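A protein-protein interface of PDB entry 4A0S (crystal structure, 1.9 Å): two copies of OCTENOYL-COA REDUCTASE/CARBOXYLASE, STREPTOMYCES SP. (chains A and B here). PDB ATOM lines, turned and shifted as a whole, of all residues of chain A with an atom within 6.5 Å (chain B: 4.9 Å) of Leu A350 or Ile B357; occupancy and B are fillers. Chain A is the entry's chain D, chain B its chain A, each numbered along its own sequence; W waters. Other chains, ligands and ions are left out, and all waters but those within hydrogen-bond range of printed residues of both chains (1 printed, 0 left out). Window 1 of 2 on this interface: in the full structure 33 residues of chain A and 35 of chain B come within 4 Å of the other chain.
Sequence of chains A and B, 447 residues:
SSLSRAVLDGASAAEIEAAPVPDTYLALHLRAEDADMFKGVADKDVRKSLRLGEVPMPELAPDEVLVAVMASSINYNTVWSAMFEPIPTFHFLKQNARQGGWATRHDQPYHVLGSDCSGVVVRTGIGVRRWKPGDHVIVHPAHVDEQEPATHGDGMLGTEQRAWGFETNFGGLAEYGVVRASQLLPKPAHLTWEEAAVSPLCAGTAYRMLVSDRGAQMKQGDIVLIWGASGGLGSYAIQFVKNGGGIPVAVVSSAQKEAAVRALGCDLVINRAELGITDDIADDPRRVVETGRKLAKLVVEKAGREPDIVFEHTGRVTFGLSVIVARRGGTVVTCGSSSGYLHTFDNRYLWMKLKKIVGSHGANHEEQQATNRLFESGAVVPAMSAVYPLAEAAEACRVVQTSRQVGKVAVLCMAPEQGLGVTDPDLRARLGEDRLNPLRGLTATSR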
ATOM      1  N   PHE A 319     -12.728   5.671  27.382  1.00  0.00           N
ATOM      2  CA  PHE A 319     -14.186   5.668  27.436  1.00  0.00           C
ATOM      3  C   PHE A 319     -14.818   7.007  27.817  1.00  0.00           C
ATOM      4  O   PHE A 319     -15.835   7.399  27.252  1.00  0.00           O
ATOM      5  CB  PHE A 319     -14.719   4.549  28.316  1.00  0.00           C
ATOM      6  CG  PHE A 319     -16.194   4.355  28.185  1.00  0.00           C
ATOM      7  CD1 PHE A 319     -16.711   3.592  27.149  1.00  0.00           C
ATOM      8  CD2 PHE A 319     -17.074   4.964  29.071  1.00  0.00           C
ATOM      9  CE1 PHE A 319     -18.079   3.398  27.021  1.00  0.00           C
ATOM     10  CE2 PHE A 319     -18.445   4.781  28.928  1.00  0.00           C
ATOM     11  CZ  PHE A 319     -18.938   3.998  27.898  1.00  0.00           C
ATOM     12  N   VAL A 323     -17.441   9.136  25.404  1.00  0.00           N
ATOM     13  CA  VAL A 323     -18.729   9.729  25.780  1.00  0.00           C
ATOM     14  C   VAL A 323     -18.748  11.228  25.457  1.00  0.00           C
ATOM     15  O   VAL A 323     -19.758  11.752  24.987  1.00  0.00           O
ATOM     16  CB  VAL A 323     -19.067   9.456  27.260  1.00  0.00           C
ATOM     17  CG1 VAL A 323     -20.288  10.281  27.721  1.00  0.00           C
ATOM     18  CG2 VAL A 323     -19.308   7.954  27.461  1.00  0.00           C
ATOM     19  N   GLY A 329     -26.655  13.002  20.593  1.00  0.00           N
ATOM     20  CA  GLY A 329     -27.436  11.869  20.135  1.00  0.00           C
ATOM     21  C   GLY A 329     -26.601  10.759  19.539  1.00  0.00           C
ATOM     22  O   GLY A 329     -27.148   9.797  19.006  1.00  0.00           O
ATOM     23  N   GLY A 330     -25.276  10.890  19.629  1.00  0.00           N
ATOM     24  CA  GLY A 330     -24.358   9.935  19.052  1.00  0.00           C
ATOM     25  C   GLY A 330     -24.296   8.675  19.881  1.00  0.00           C
ATOM     26  O   GLY A 330     -24.862   8.605  20.987  1.00  0.00           O
ATOM     27  N   VAL A 332     -21.783   5.625  21.475  1.00  0.00           N
ATOM     28  CA  VAL A 332     -20.557   4.911  21.769  1.00  0.00           C
ATOM     29  C   VAL A 332     -20.927   3.434  21.788  1.00  0.00           C
ATOM     30  O   VAL A 332     -21.739   3.015  22.588  1.00  0.00           O
ATOM     31  CB  VAL A 332     -19.970   5.312  23.143  1.00  0.00           C
ATOM     32  CG1 VAL A 332     -18.723   4.475  23.436  1.00  0.00           C
ATOM     33  CG2 VAL A 332     -19.623   6.790  23.151  1.00  0.00           C
ATOM     34  N   PHE A 345     -17.103   7.922  33.324  1.00  0.00           N
ATOM     35  CA  PHE A 345     -17.484   8.959  32.396  1.00  0.00           C
ATOM     36  C   PHE A 345     -18.348   9.983  33.087  1.00  0.00           C
ATOM     37  O   PHE A 345     -18.933   9.716  34.133  1.00  0.00           O
ATOM     38  CB  PHE A 345     -18.204   8.356  31.186  1.00  0.00           C
ATOM     39  CG  PHE A 345     -19.560   7.829  31.502  1.00  0.00           C
ATOM     40  CD1 PHE A 345     -19.724   6.543  31.997  1.00  0.00           C
ATOM     41  CD2 PHE A 345     -20.671   8.616  31.320  1.00  0.00           C
ATOM     42  CE1 PHE A 345     -20.981   6.054  32.295  1.00  0.00           C
ATOM     43  CE2 PHE A 345     -21.942   8.130  31.621  1.00  0.00           C
ATOM     44  CZ  PHE A 345     -22.095   6.861  32.117  1.00  0.00           C
ATOM     45  N   ASP A 346     -18.394  11.166  32.496  1.00  0.00           N
ATOM     46  CA  ASP A 346     -19.211  12.251  32.978  1.00  0.00           C
ATOM     47  C   ASP A 346     -20.602  12.097  32.363  1.00  0.00           C
ATOM     48  O   ASP A 346     -20.807  12.341  31.160  1.00  0.00           O
ATOM     49  CB  ASP A 346     -18.553  13.569  32.583  1.00  0.00           C
ATOM     50  CG  ASP A 346     -19.266  14.772  33.138  1.00  0.00           C
ATOM     51  OD1 ASP A 346     -20.509  14.740  33.246  1.00  0.00           O
ATOM     52  OD2 ASP A 346     -18.581  15.769  33.453  1.00  0.00           O
ATOM     53  N   ASN A 347     -21.553  11.674  33.188  1.00  0.00           N
ATOM     54  CA  ASN A 347     -22.891  11.373  32.700  1.00  0.00           C
ATOM     55  C   ASN A 347     -23.607  12.568  32.098  1.00  0.00           C
ATOM     56  O   ASN A 347     -24.456  12.387  31.234  1.00  0.00           O
ATOM     57  CB  ASN A 347     -23.768  10.715  33.771  1.00  0.00           C
ATOM     58  CG  ASN A 347     -25.018  10.064  33.178  1.00  0.00           C
ATOM     59  OD1 ASN A 347     -24.940   9.395  32.159  1.00  0.00           O
ATOM     60  ND2 ASN A 347     -26.164  10.275  33.806  1.00  0.00           N
ATOM     61  N   ARG A 348     -23.262  13.782  32.540  1.00  0.00           N
ATOM     62  CA  ARG A 348     -23.808  14.993  31.937  1.00  0.00           C
ATOM     63  C   ARG A 348     -23.640  14.966  30.417  1.00  0.00           C
ATOM     64  O   ARG A 348     -24.551  15.312  29.675  1.00  0.00           O
ATOM     65  CB  ARG A 348     -23.138  16.241  32.503  1.00  0.00           C
ATOM     66  CG  ARG A 348     -23.360  16.441  33.979  1.00  0.00           C
ATOM     67  CD  ARG A 348     -22.583  17.628  34.447  1.00  0.00           C
ATOM     68  NE  ARG A 348     -21.147  17.453  34.238  1.00  0.00           N
ATOM     69  CZ  ARG A 348     -20.267  18.448  34.234  1.00  0.00           C
ATOM     70  NH1 ARG A 348     -20.680  19.700  34.423  1.00  0.00           N
ATOM     71  NH2 ARG A 348     -18.975  18.196  34.032  1.00  0.00           N
ATOM     72  N   TYR A 349     -22.474  14.521  29.963  1.00  0.00           N
ATOM     73  CA  TYR A 349     -22.206  14.415  28.534  1.00  0.00           C
ATOM     74  C   TYR A 349     -23.131  13.400  27.872  1.00  0.00           C
ATOM     75  O   TYR A 349     -23.533  13.569  26.713  1.00  0.00           O
ATOM     76  CB  TYR A 349     -20.710  14.133  28.274  1.00  0.00           C
ATOM     77  CG  TYR A 349     -19.915  15.386  28.542  1.00  0.00           C
ATOM     78  CD1 TYR A 349     -19.718  16.343  27.549  1.00  0.00           C
ATOM     79  CD2 TYR A 349     -19.438  15.659  29.824  1.00  0.00           C
ATOM     80  CE1 TYR A 349     -19.029  17.541  27.832  1.00  0.00           C
ATOM     81  CE2 TYR A 349     -18.757  16.845  30.116  1.00  0.00           C
ATOM     82  CZ  TYR A 349     -18.545  17.772  29.123  1.00  0.00           C
ATOM     83  OH  TYR A 349     -17.863  18.940  29.446  1.00  0.00           O
ATOM     84  N   LEU A 350     -23.512  12.382  28.628  1.00  0.00           N
ATOM     85  CA  LEU A 350     -24.322  11.318  28.074  1.00  0.00           C
ATOM     86  C   LEU A 350     -25.771  11.738  28.020  1.00  0.00           C
ATOM     87  O   LEU A 350     -26.337  11.831  26.931  1.00  0.00           O
ATOM     88  CB  LEU A 350     -24.166  10.018  28.852  1.00  0.00           C
ATOM     89  CG  LEU A 350     -24.984   8.878  28.241  1.00  0.00           C
ATOM     90  CD1 LEU A 350     -24.195   8.270  27.111  1.00  0.00           C
ATOM     91  CD2 LEU A 350     -25.241   7.875  29.310  1.00  0.00           C
ATOM     92  N   TRP A 351     -26.367  12.020  29.173  1.00  0.00           N
ATOM     93  CA  TRP A 351     -27.800  12.318  29.177  1.00  0.00           C
ATOM     94  C   TRP A 351     -28.095  13.670  28.552  1.00  0.00           C
ATOM     95  O   TRP A 351     -29.041  13.793  27.784  1.00  0.00           O
ATOM     96  CB  TRP A 351     -28.427  12.189  30.583  1.00  0.00           C
ATOM     97  CG  TRP A 351     -28.575  13.493  31.317  1.00  0.00           C
ATOM     98  CD1 TRP A 351     -29.463  14.506  31.033  1.00  0.00           C
ATOM     99  CD2 TRP A 351     -27.840  13.921  32.469  1.00  0.00           C
ATOM    100  NE1 TRP A 351     -29.296  15.552  31.922  1.00  0.00           N
ATOM    101  CE2 TRP A 351     -28.324  15.213  32.823  1.00  0.00           C
ATOM    102  CE3 TRP A 351     -26.815  13.348  33.237  1.00  0.00           C
ATOM    103  CZ2 TRP A 351     -27.804  15.938  33.896  1.00  0.00           C
ATOM    104  CZ3 TRP A 351     -26.308  14.067  34.309  1.00  0.00           C
ATOM    105  CH2 TRP A 351     -26.806  15.352  34.633  1.00  0.00           C
ATOM    106  N   MET A 352     -27.275  14.680  28.852  1.00  0.00           N
ATOM    107  CA  MET A 352     -27.605  16.042  28.413  1.00  0.00           C
ATOM    108  C   MET A 352     -27.586  16.116  26.905  1.00  0.00           C
ATOM    109  O   MET A 352     -28.301  16.908  26.311  1.00  0.00           O
ATOM    110  CB  MET A 352     -26.647  17.095  28.967  1.00  0.00           C
ATOM    111  CG  MET A 352     -26.830  17.415  30.437  1.00  0.00           C
ATOM    112  SD  MET A 352     -28.350  18.355  30.642  1.00  0.00           S
ATOM    113  CE  MET A 352     -27.957  19.936  29.870  1.00  0.00           C
ATOM    114  N   LYS A 353     -26.773  15.271  26.292  1.00  0.00           N
ATOM    115  CA  LYS A 353     -26.622  15.287  24.831  1.00  0.00           C
ATOM    116  C   LYS A 353     -27.289  14.084  24.181  1.00  0.00           C
ATOM    117  O   LYS A 353     -27.119  13.817  22.987  1.00  0.00           O
ATOM    118  CB  LYS A 353     -25.152  15.457  24.449  1.00  0.00           C
ATOM    119  CG  LYS A 353     -24.580  16.690  25.170  1.00  0.00           C
ATOM    120  CD  LYS A 353     -23.233  17.125  24.690  1.00  0.00           C
ATOM    121  CE  LYS A 353     -22.890  18.502  25.274  1.00  0.00           C
ATOM    122  NZ  LYS A 353     -23.964  19.507  25.008  1.00  0.00           N
ATOM    123  N   LEU A 354     -28.120  13.421  24.984  1.00  0.00           N
ATOM    124  CA  LEU A 354     -28.874  12.257  24.575  1.00  0.00           C
ATOM    125  C   LEU A 354     -28.026  11.238  23.835  1.00  0.00           C
ATOM    126  O   LEU A 354     -28.449  10.709  22.799  1.00  0.00           O
ATOM    127  CB  LEU A 354     -30.105  12.634  23.738  1.00  0.00           C
ATOM    128  CG  LEU A 354     -30.960  13.638  24.488  1.00  0.00           C
ATOM    129  CD1 LEU A 354     -30.722  15.085  24.020  1.00  0.00           C
ATOM    130  CD2 LEU A 354     -32.425  13.246  24.442  1.00  0.00           C
ATOM    131  N   LYS A 355     -26.848  10.937  24.377  1.00  0.00           N
ATOM    132  CA  LYS A 355     -26.007   9.950  23.739  1.00  0.00           C
ATOM    133  C   LYS A 355     -26.339   8.568  24.270  1.00  0.00           C
ATOM    134  O   LYS A 355     -27.041   8.430  25.257  1.00  0.00           O
ATOM    135  CB  LYS A 355     -24.538  10.270  23.961  1.00  0.00           C
ATOM    136  CG  LYS A 355     -24.176  11.708  23.606  1.00  0.00           C
ATOM    137  CD  LYS A 355     -22.691  11.929  23.803  1.00  0.00           C
ATOM    138  CE  LYS A 355     -22.381  13.427  23.791  1.00  0.00           C
ATOM    139  NZ  LYS A 355     -20.934  13.702  23.739  1.00  0.00           N
ATOM    140  N   LYS A 356     -25.820   7.552  23.606  1.00  0.00           N
ATOM    141  CA  LYS A 356     -26.096   6.191  23.990  1.00  0.00           C
ATOM    142  C   LYS A 356     -24.798   5.452  24.043  1.00  0.00           C
ATOM    143  O   LYS A 356     -23.858   5.738  23.294  1.00  0.00           O
ATOM    144  CB  LYS A 356     -26.949   5.506  22.935  1.00  0.00           C
ATOM    145  CG  LYS A 356     -28.374   5.919  22.925  1.00  0.00           C
ATOM    146  CD  LYS A 356     -29.057   5.373  21.654  1.00  0.00           C
ATOM    147  CE  LYS A 356     -28.638   6.136  20.382  1.00  0.00           C
ATOM    148  NZ  LYS A 356     -28.174   7.544  20.637  1.00  0.00           N
ATOM    149  N   ILE A 357     -24.745   4.499  24.950  1.00  0.00           N
ATOM    150  CA  ILE A 357     -23.679   3.544  24.952  1.00  0.00           C
ATOM    151  C   ILE A 357     -24.313   2.204  24.695  1.00  0.00           C
ATOM    152  O   ILE A 357     -25.154   1.744  25.463  1.00  0.00           O
ATOM    153  CB  ILE A 357     -22.900   3.544  26.263  1.00  0.00           C
ATOM    154  CG1 ILE A 357     -22.347   4.961  26.502  1.00  0.00           C
ATOM    155  CG2 ILE A 357     -21.785   2.541  26.191  1.00  0.00           C
ATOM    156  CD1 ILE A 357     -22.127   5.265  27.958  1.00  0.00           C
ATOM    157  N   VAL A 358     -23.914   1.607  23.587  1.00  0.00           N
ATOM    158  CA  VAL A 358     -24.398   0.300  23.200  1.00  0.00           C
ATOM    159  C   VAL A 358     -23.307  -0.719  23.468  1.00  0.00           C
ATOM    160  O   VAL A 358     -22.231  -0.672  22.875  1.00  0.00           O
ATOM    161  CB  VAL A 358     -24.804   0.273  21.723  1.00  0.00           C
ATOM    162  CG1 VAL A 358     -25.295  -1.111  21.324  1.00  0.00           C
ATOM    163  CG2 VAL A 358     -25.892   1.303  21.467  1.00  0.00           C
ATOM    164  N   GLY A 359     -23.604  -1.609  24.401  1.00  0.00           N
ATOM    165  CA  GLY A 359     -22.739  -2.703  24.727  1.00  0.00           C
ATOM    166  C   GLY A 359     -22.977  -3.686  23.607  1.00  0.00           C
ATOM    167  O   GLY A 359     -24.126  -4.000  23.273  1.00  0.00           O
ATOM    168  N   PHE B 319     -25.296   3.984  39.635  1.00  0.00           N
ATOM    169  CA  PHE B 319     -25.169   3.673  38.220  1.00  0.00           C
ATOM    170  C   PHE B 319     -24.451   2.362  37.954  1.00  0.00           C
ATOM    171  O   PHE B 319     -24.848   1.623  37.071  1.00  0.00           O
ATOM    172  CB  PHE B 319     -24.504   4.798  37.451  1.00  0.00           C
ATOM    173  CG  PHE B 319     -24.533   4.591  35.974  1.00  0.00           C
ATOM    174  CD1 PHE B 319     -25.638   4.968  35.239  1.00  0.00           C
ATOM    175  CD2 PHE B 319     -23.469   3.986  35.324  1.00  0.00           C
ATOM    176  CE1 PHE B 319     -25.685   4.772  33.871  1.00  0.00           C
ATOM    177  CE2 PHE B 319     -23.517   3.776  33.943  1.00  0.00           C
ATOM    178  CZ  PHE B 319     -24.628   4.162  33.231  1.00  0.00           C
ATOM    179  N   VAL B 323     -26.025  -0.804  35.831  1.00  0.00           N
ATOM    180  CA  VAL B 323     -25.380  -1.579  34.775  1.00  0.00           C
ATOM    181  C   VAL B 323     -25.360  -3.072  35.103  1.00  0.00           C
ATOM    182  O   VAL B 323     -25.610  -3.913  34.242  1.00  0.00           O
ATOM    183  CB  VAL B 323     -23.941  -1.074  34.479  1.00  0.00           C
ATOM    184  CG1 VAL B 323     -23.242  -2.011  33.538  1.00  0.00           C
ATOM    185  CG2 VAL B 323     -24.001   0.286  33.851  1.00  0.00           C
ATOM    186  N   VAL B 332     -30.116   0.559  30.619  1.00  0.00           N
ATOM    187  CA  VAL B 332     -30.087   1.549  31.654  1.00  0.00           C
ATOM    188  C   VAL B 332     -30.386   2.856  30.923  1.00  0.00           C
ATOM    189  O   VAL B 332     -29.646   3.249  30.030  1.00  0.00           O
ATOM    190  CB  VAL B 332     -28.709   1.633  32.320  1.00  0.00           C
ATOM    191  CG1 VAL B 332     -28.714   2.743  33.364  1.00  0.00           C
ATOM    192  CG2 VAL B 332     -28.329   0.303  32.932  1.00  0.00           C
ATOM    193  N   THR B 334     -30.824   6.840  31.458  1.00  0.00           N
ATOM    194  CA  THR B 334     -30.451   7.817  32.468  1.00  0.00           C
ATOM    195  C   THR B 334     -30.692   9.233  31.988  1.00  0.00           C
ATOM    196  O   THR B 334     -30.399   9.560  30.830  1.00  0.00           O
ATOM    197  CB  THR B 334     -28.961   7.692  32.869  1.00  0.00           C
ATOM    198  OG1 THR B 334     -28.639   8.723  33.811  1.00  0.00           O
ATOM    199  CG2 THR B 334     -28.046   7.802  31.641  1.00  0.00           C
ATOM    200  N   PHE B 345     -18.640   2.335  36.164  1.00  0.00           N
ATOM    201  CA  PHE B 345     -19.321   1.088  35.990  1.00  0.00           C
ATOM    202  C   PHE B 345     -18.337   0.091  35.415  1.00  0.00           C
ATOM    203  O   PHE B 345     -17.311   0.459  34.830  1.00  0.00           O
ATOM    204  CB  PHE B 345     -20.554   1.247  35.084  1.00  0.00           C
ATOM    205  CG  PHE B 345     -20.223   1.480  33.638  1.00  0.00           C
ATOM    206  CD1 PHE B 345     -19.945   2.761  33.175  1.00  0.00           C
ATOM    207  CD2 PHE B 345     -20.165   0.417  32.744  1.00  0.00           C
ATOM    208  CE1 PHE B 345     -19.623   2.988  31.824  1.00  0.00           C
ATOM    209  CE2 PHE B 345     -19.849   0.630  31.397  1.00  0.00           C
ATOM    210  CZ  PHE B 345     -19.574   1.915  30.939  1.00  0.00           C
ATOM    211  N   LEU B 350     -21.643  -4.439  30.718  1.00  0.00           N
ATOM    212  CA  LEU B 350     -22.276  -3.768  29.606  1.00  0.00           C
ATOM    213  C   LEU B 350     -22.104  -4.531  28.292  1.00  0.00           C
ATOM    214  O   LEU B 350     -23.091  -4.876  27.642  1.00  0.00           O
ATOM    215  CB  LEU B 350     -21.755  -2.350  29.455  1.00  0.00           C
ATOM    216  CG  LEU B 350     -22.687  -1.543  28.561  1.00  0.00           C
ATOM    217  CD1 LEU B 350     -23.929  -1.163  29.367  1.00  0.00           C
ATOM    218  CD2 LEU B 350     -21.968  -0.321  28.122  1.00  0.00           C
ATOM    219  N   LYS B 355     -25.745  -5.017  27.067  1.00  0.00           N
ATOM    220  CA  LYS B 355     -26.646  -4.030  27.645  1.00  0.00           C
ATOM    221  C   LYS B 355     -26.438  -2.669  26.978  1.00  0.00           C
ATOM    222  O   LYS B 355     -25.412  -2.424  26.347  1.00  0.00           O
ATOM    223  CB  LYS B 355     -26.408  -3.915  29.146  1.00  0.00           C
ATOM    224  CG  LYS B 355     -26.410  -5.265  29.848  1.00  0.00           C
ATOM    225  CD  LYS B 355     -26.426  -5.097  31.348  1.00  0.00           C
ATOM    226  CE  LYS B 355     -26.196  -6.435  32.052  1.00  0.00           C
ATOM    227  NZ  LYS B 355     -26.252  -6.244  33.533  1.00  0.00           N
ATOM    228  N   LYS B 356     -27.413  -1.789  27.144  1.00  0.00           N
ATOM    229  CA  LYS B 356     -27.330  -0.452  26.599  1.00  0.00           C
ATOM    230  C   LYS B 356     -27.516   0.548  27.714  1.00  0.00           C
ATOM    231  O   LYS B 356     -28.281   0.323  28.650  1.00  0.00           O
ATOM    232  CB  LYS B 356     -28.439  -0.210  25.581  1.00  0.00           C
ATOM    233  CG  LYS B 356     -28.444  -1.127  24.396  1.00  0.00           C
ATOM    234  CD  LYS B 356     -29.409  -0.588  23.324  1.00  0.00           C
ATOM    235  CE  LYS B 356     -30.866  -1.050  23.530  1.00  0.00           C
ATOM    236  NZ  LYS B 356     -31.707  -0.053  24.292  1.00  0.00           N
ATOM    237  N   ILE B 357     -26.831   1.671  27.581  1.00  0.00           N
ATOM    238  CA  ILE B 357     -27.090   2.816  28.409  1.00  0.00           C
ATOM    239  C   ILE B 357     -27.596   3.895  27.487  1.00  0.00           C
ATOM    240  O   ILE B 357     -26.894   4.320  26.570  1.00  0.00           O
ATOM    241  CB  ILE B 357     -25.842   3.344  29.117  1.00  0.00           C
ATOM    242  CG1 ILE B 357     -25.177   2.262  29.957  1.00  0.00           C
ATOM    243  CG2 ILE B 357     -26.221   4.539  29.999  1.00  0.00           C
ATOM    244  CD1 ILE B 357     -23.685   2.507  30.173  1.00  0.00           C
ATOM    245  N   VAL B 358     -28.818   4.330  27.736  1.00  0.00           N
ATOM    246  CA  VAL B 358     -29.428   5.349  26.923  1.00  0.00           C
ATOM    247  C   VAL B 358     -29.489   6.636  27.726  1.00  0.00           C
ATOM    248  O   VAL B 358     -30.141   6.700  28.758  1.00  0.00           O
ATOM    249  CB  VAL B 358     -30.818   4.924  26.428  1.00  0.00           C
ATOM    250  CG1 VAL B 358     -31.444   6.043  25.579  1.00  0.00           C
ATOM    251  CG2 VAL B 358     -30.701   3.614  25.630  1.00  0.00           C
ATOM    252  N   GLY B 359     -28.752   7.632  27.253  1.00  0.00           N
ATOM    253  CA  GLY B 359     -28.770   8.952  27.855  1.00  0.00           C
ATOM    254  C   GLY B 359     -30.036   9.586  27.339  1.00  0.00           C
ATOM    255  O   GLY B 359     -30.327   9.512  26.149  1.00  0.00           O
HETATM  256  O   HOH W   1     -30.274   8.463  23.805  1.00  0.00           O
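ND2 of Asn A347 sits at hydrogen-bond distance from OG1 of Thr B334 (2.9 Å).
N of Gly A359 lies within hydrogen-bond range of O of Lys B355, at 2.8 Å.
The backbone carbonyl oxygen (O) of Ile B357 is in hydrogen-bond range of the backbone NH (N) of Ile A357 (2.7 Å).
N of Gly B359 lies within hydrogen-bond range of O of Lys A355, at 2.7 Å.
O of Lys B356 lies within hydrogen-bond range of N of Val B332 (2.7 Å).
The backbone NH of Val B358 sits at hydrogen-bond distance from the backbone carbonyl oxygen of Val B332.
The backbone NH of Thr B334 sits at hydrogen-bond distance from the backbone carbonyl oxygen of Val B358 (2.8 Å).
O of Leu B350 lies within hydrogen-bond range of N of Lys B355, at 2.7 Å.
The backbone carbonyl oxygen of Lys A356 lies within hydrogen-bond range of the backbone NH of Val A332 (2.8 Å).
The backbone NH of Val A358 lies within hydrogen-bond range of the backbone carbonyl oxygen of Val A332, 2.8 Å away.
Among the printed residues, pairs that only touch across the chains: Phe A319 with Phe B345 (3.6 Å), Phe A345 with Phe B319 (3.8 Å), Phe A345 with Phe B345 (3.4 Å), Leu A350 with Thr B334 (3.6 Å), Leu A350 with Ile B357 (3.5 Å), Leu A350 with Gly B359 (3.8 Å), Trp A351 with Thr B334 (3.3 Å), Trp A351 with Gly B359 (3.7 Å), Leu A354 with Gly B359 (3.5 Å), Lys A355 with Val B358 (3.9 Å), Lys A356 with Ile B357 (3.3 Å), Ile A357 with Leu B350 (3.5 Å), Ile A357 with Lys B356 (3.3 Å), Val A358 with Lys B355 (3.95 Å) and Gly A359 with Leu B350 (3.7 Å).
Of chain B, only Thr B334 (3.6 Å), Ile B357 (3.5 Å) and Gly B359 (3.8 Å) come within 4 Å of Leu A350.
Printed residues of chain B within 4 Å of Gly A359: Leu B350 (3.7 Å) and Lys B355 (2.8 Å).
Of the printed residues of chain A, Phe B319 touches Phe A345 (3.8 Å).
Of the printed residues of chain A, Lys B355 touches Val A358 and Gly A359.
Of chain A, only Leu A350 (3.5 Å), Lys A356 (3.3 Å) and Ile A357 (2.7 Å) come within 4 Å of Ile B357.
Of the printed residues of chain A, Gly B359 touches Leu A350 (3.8 Å), Trp A351 (3.7 Å), Leu A354 (3.5 Å) and Lys A355 (2.7 Å).
The nearest residue of chain A that does not touch Ile B357 is Lys A355 (4.3 Å).
The nearest printed residue of chain B that does not touch Asn A347 is Phe B319 (5.0 Å).
Printed residues of chain A that touch a printed residue of chain B: Phe A319, Phe A345, Asn A347, Leu A350, Trp A351, Leu A354, Lys A355, Lys A356, Ile A357, Val A358 and Gly A359.
Printed residues of chain B that touch a printed residue of chain A: Phe B319, Thr B334, Phe B345, Leu B350, Lys B355, Lys B356, Ile B357, Val B358 and Gly B359.
Hydrophobic or aromatic side chains of chain B that line the printed part of chain A: Phe B319, Phe B345, Leu B350 and Ile B357.
Among the printed residues, no Asp or Glu carboxylate lies within 4 Å of a Lys or Arg side-chain nitrogen of the other chain.
Phe A319 touches Phe B345, and with the chains exchanged Phe A345 touches Phe B319.
Phe B345 touches its own counterpart, Phe A345.
Leu A350 touches Ile B357, and with the chains exchanged Ile A357 touches Leu B350.
Lys A356 touches Ile B357, and with the chains exchanged Ile A357 touches Lys B356.
Positions printed for both chains: 319, 323, 332, 345, 350, 355, 356, 357, 358 and 359.
Of the 19 pairs that touch across the chains among the printed residues, 14 have their exchanged pair printed and touching as well.
Water W1 bridges the backbone carbonyl oxygen (O) of Gly B359 (2.6 Å) and the backbone carbonyl oxygen (O) of Leu A354 (3.1 Å).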
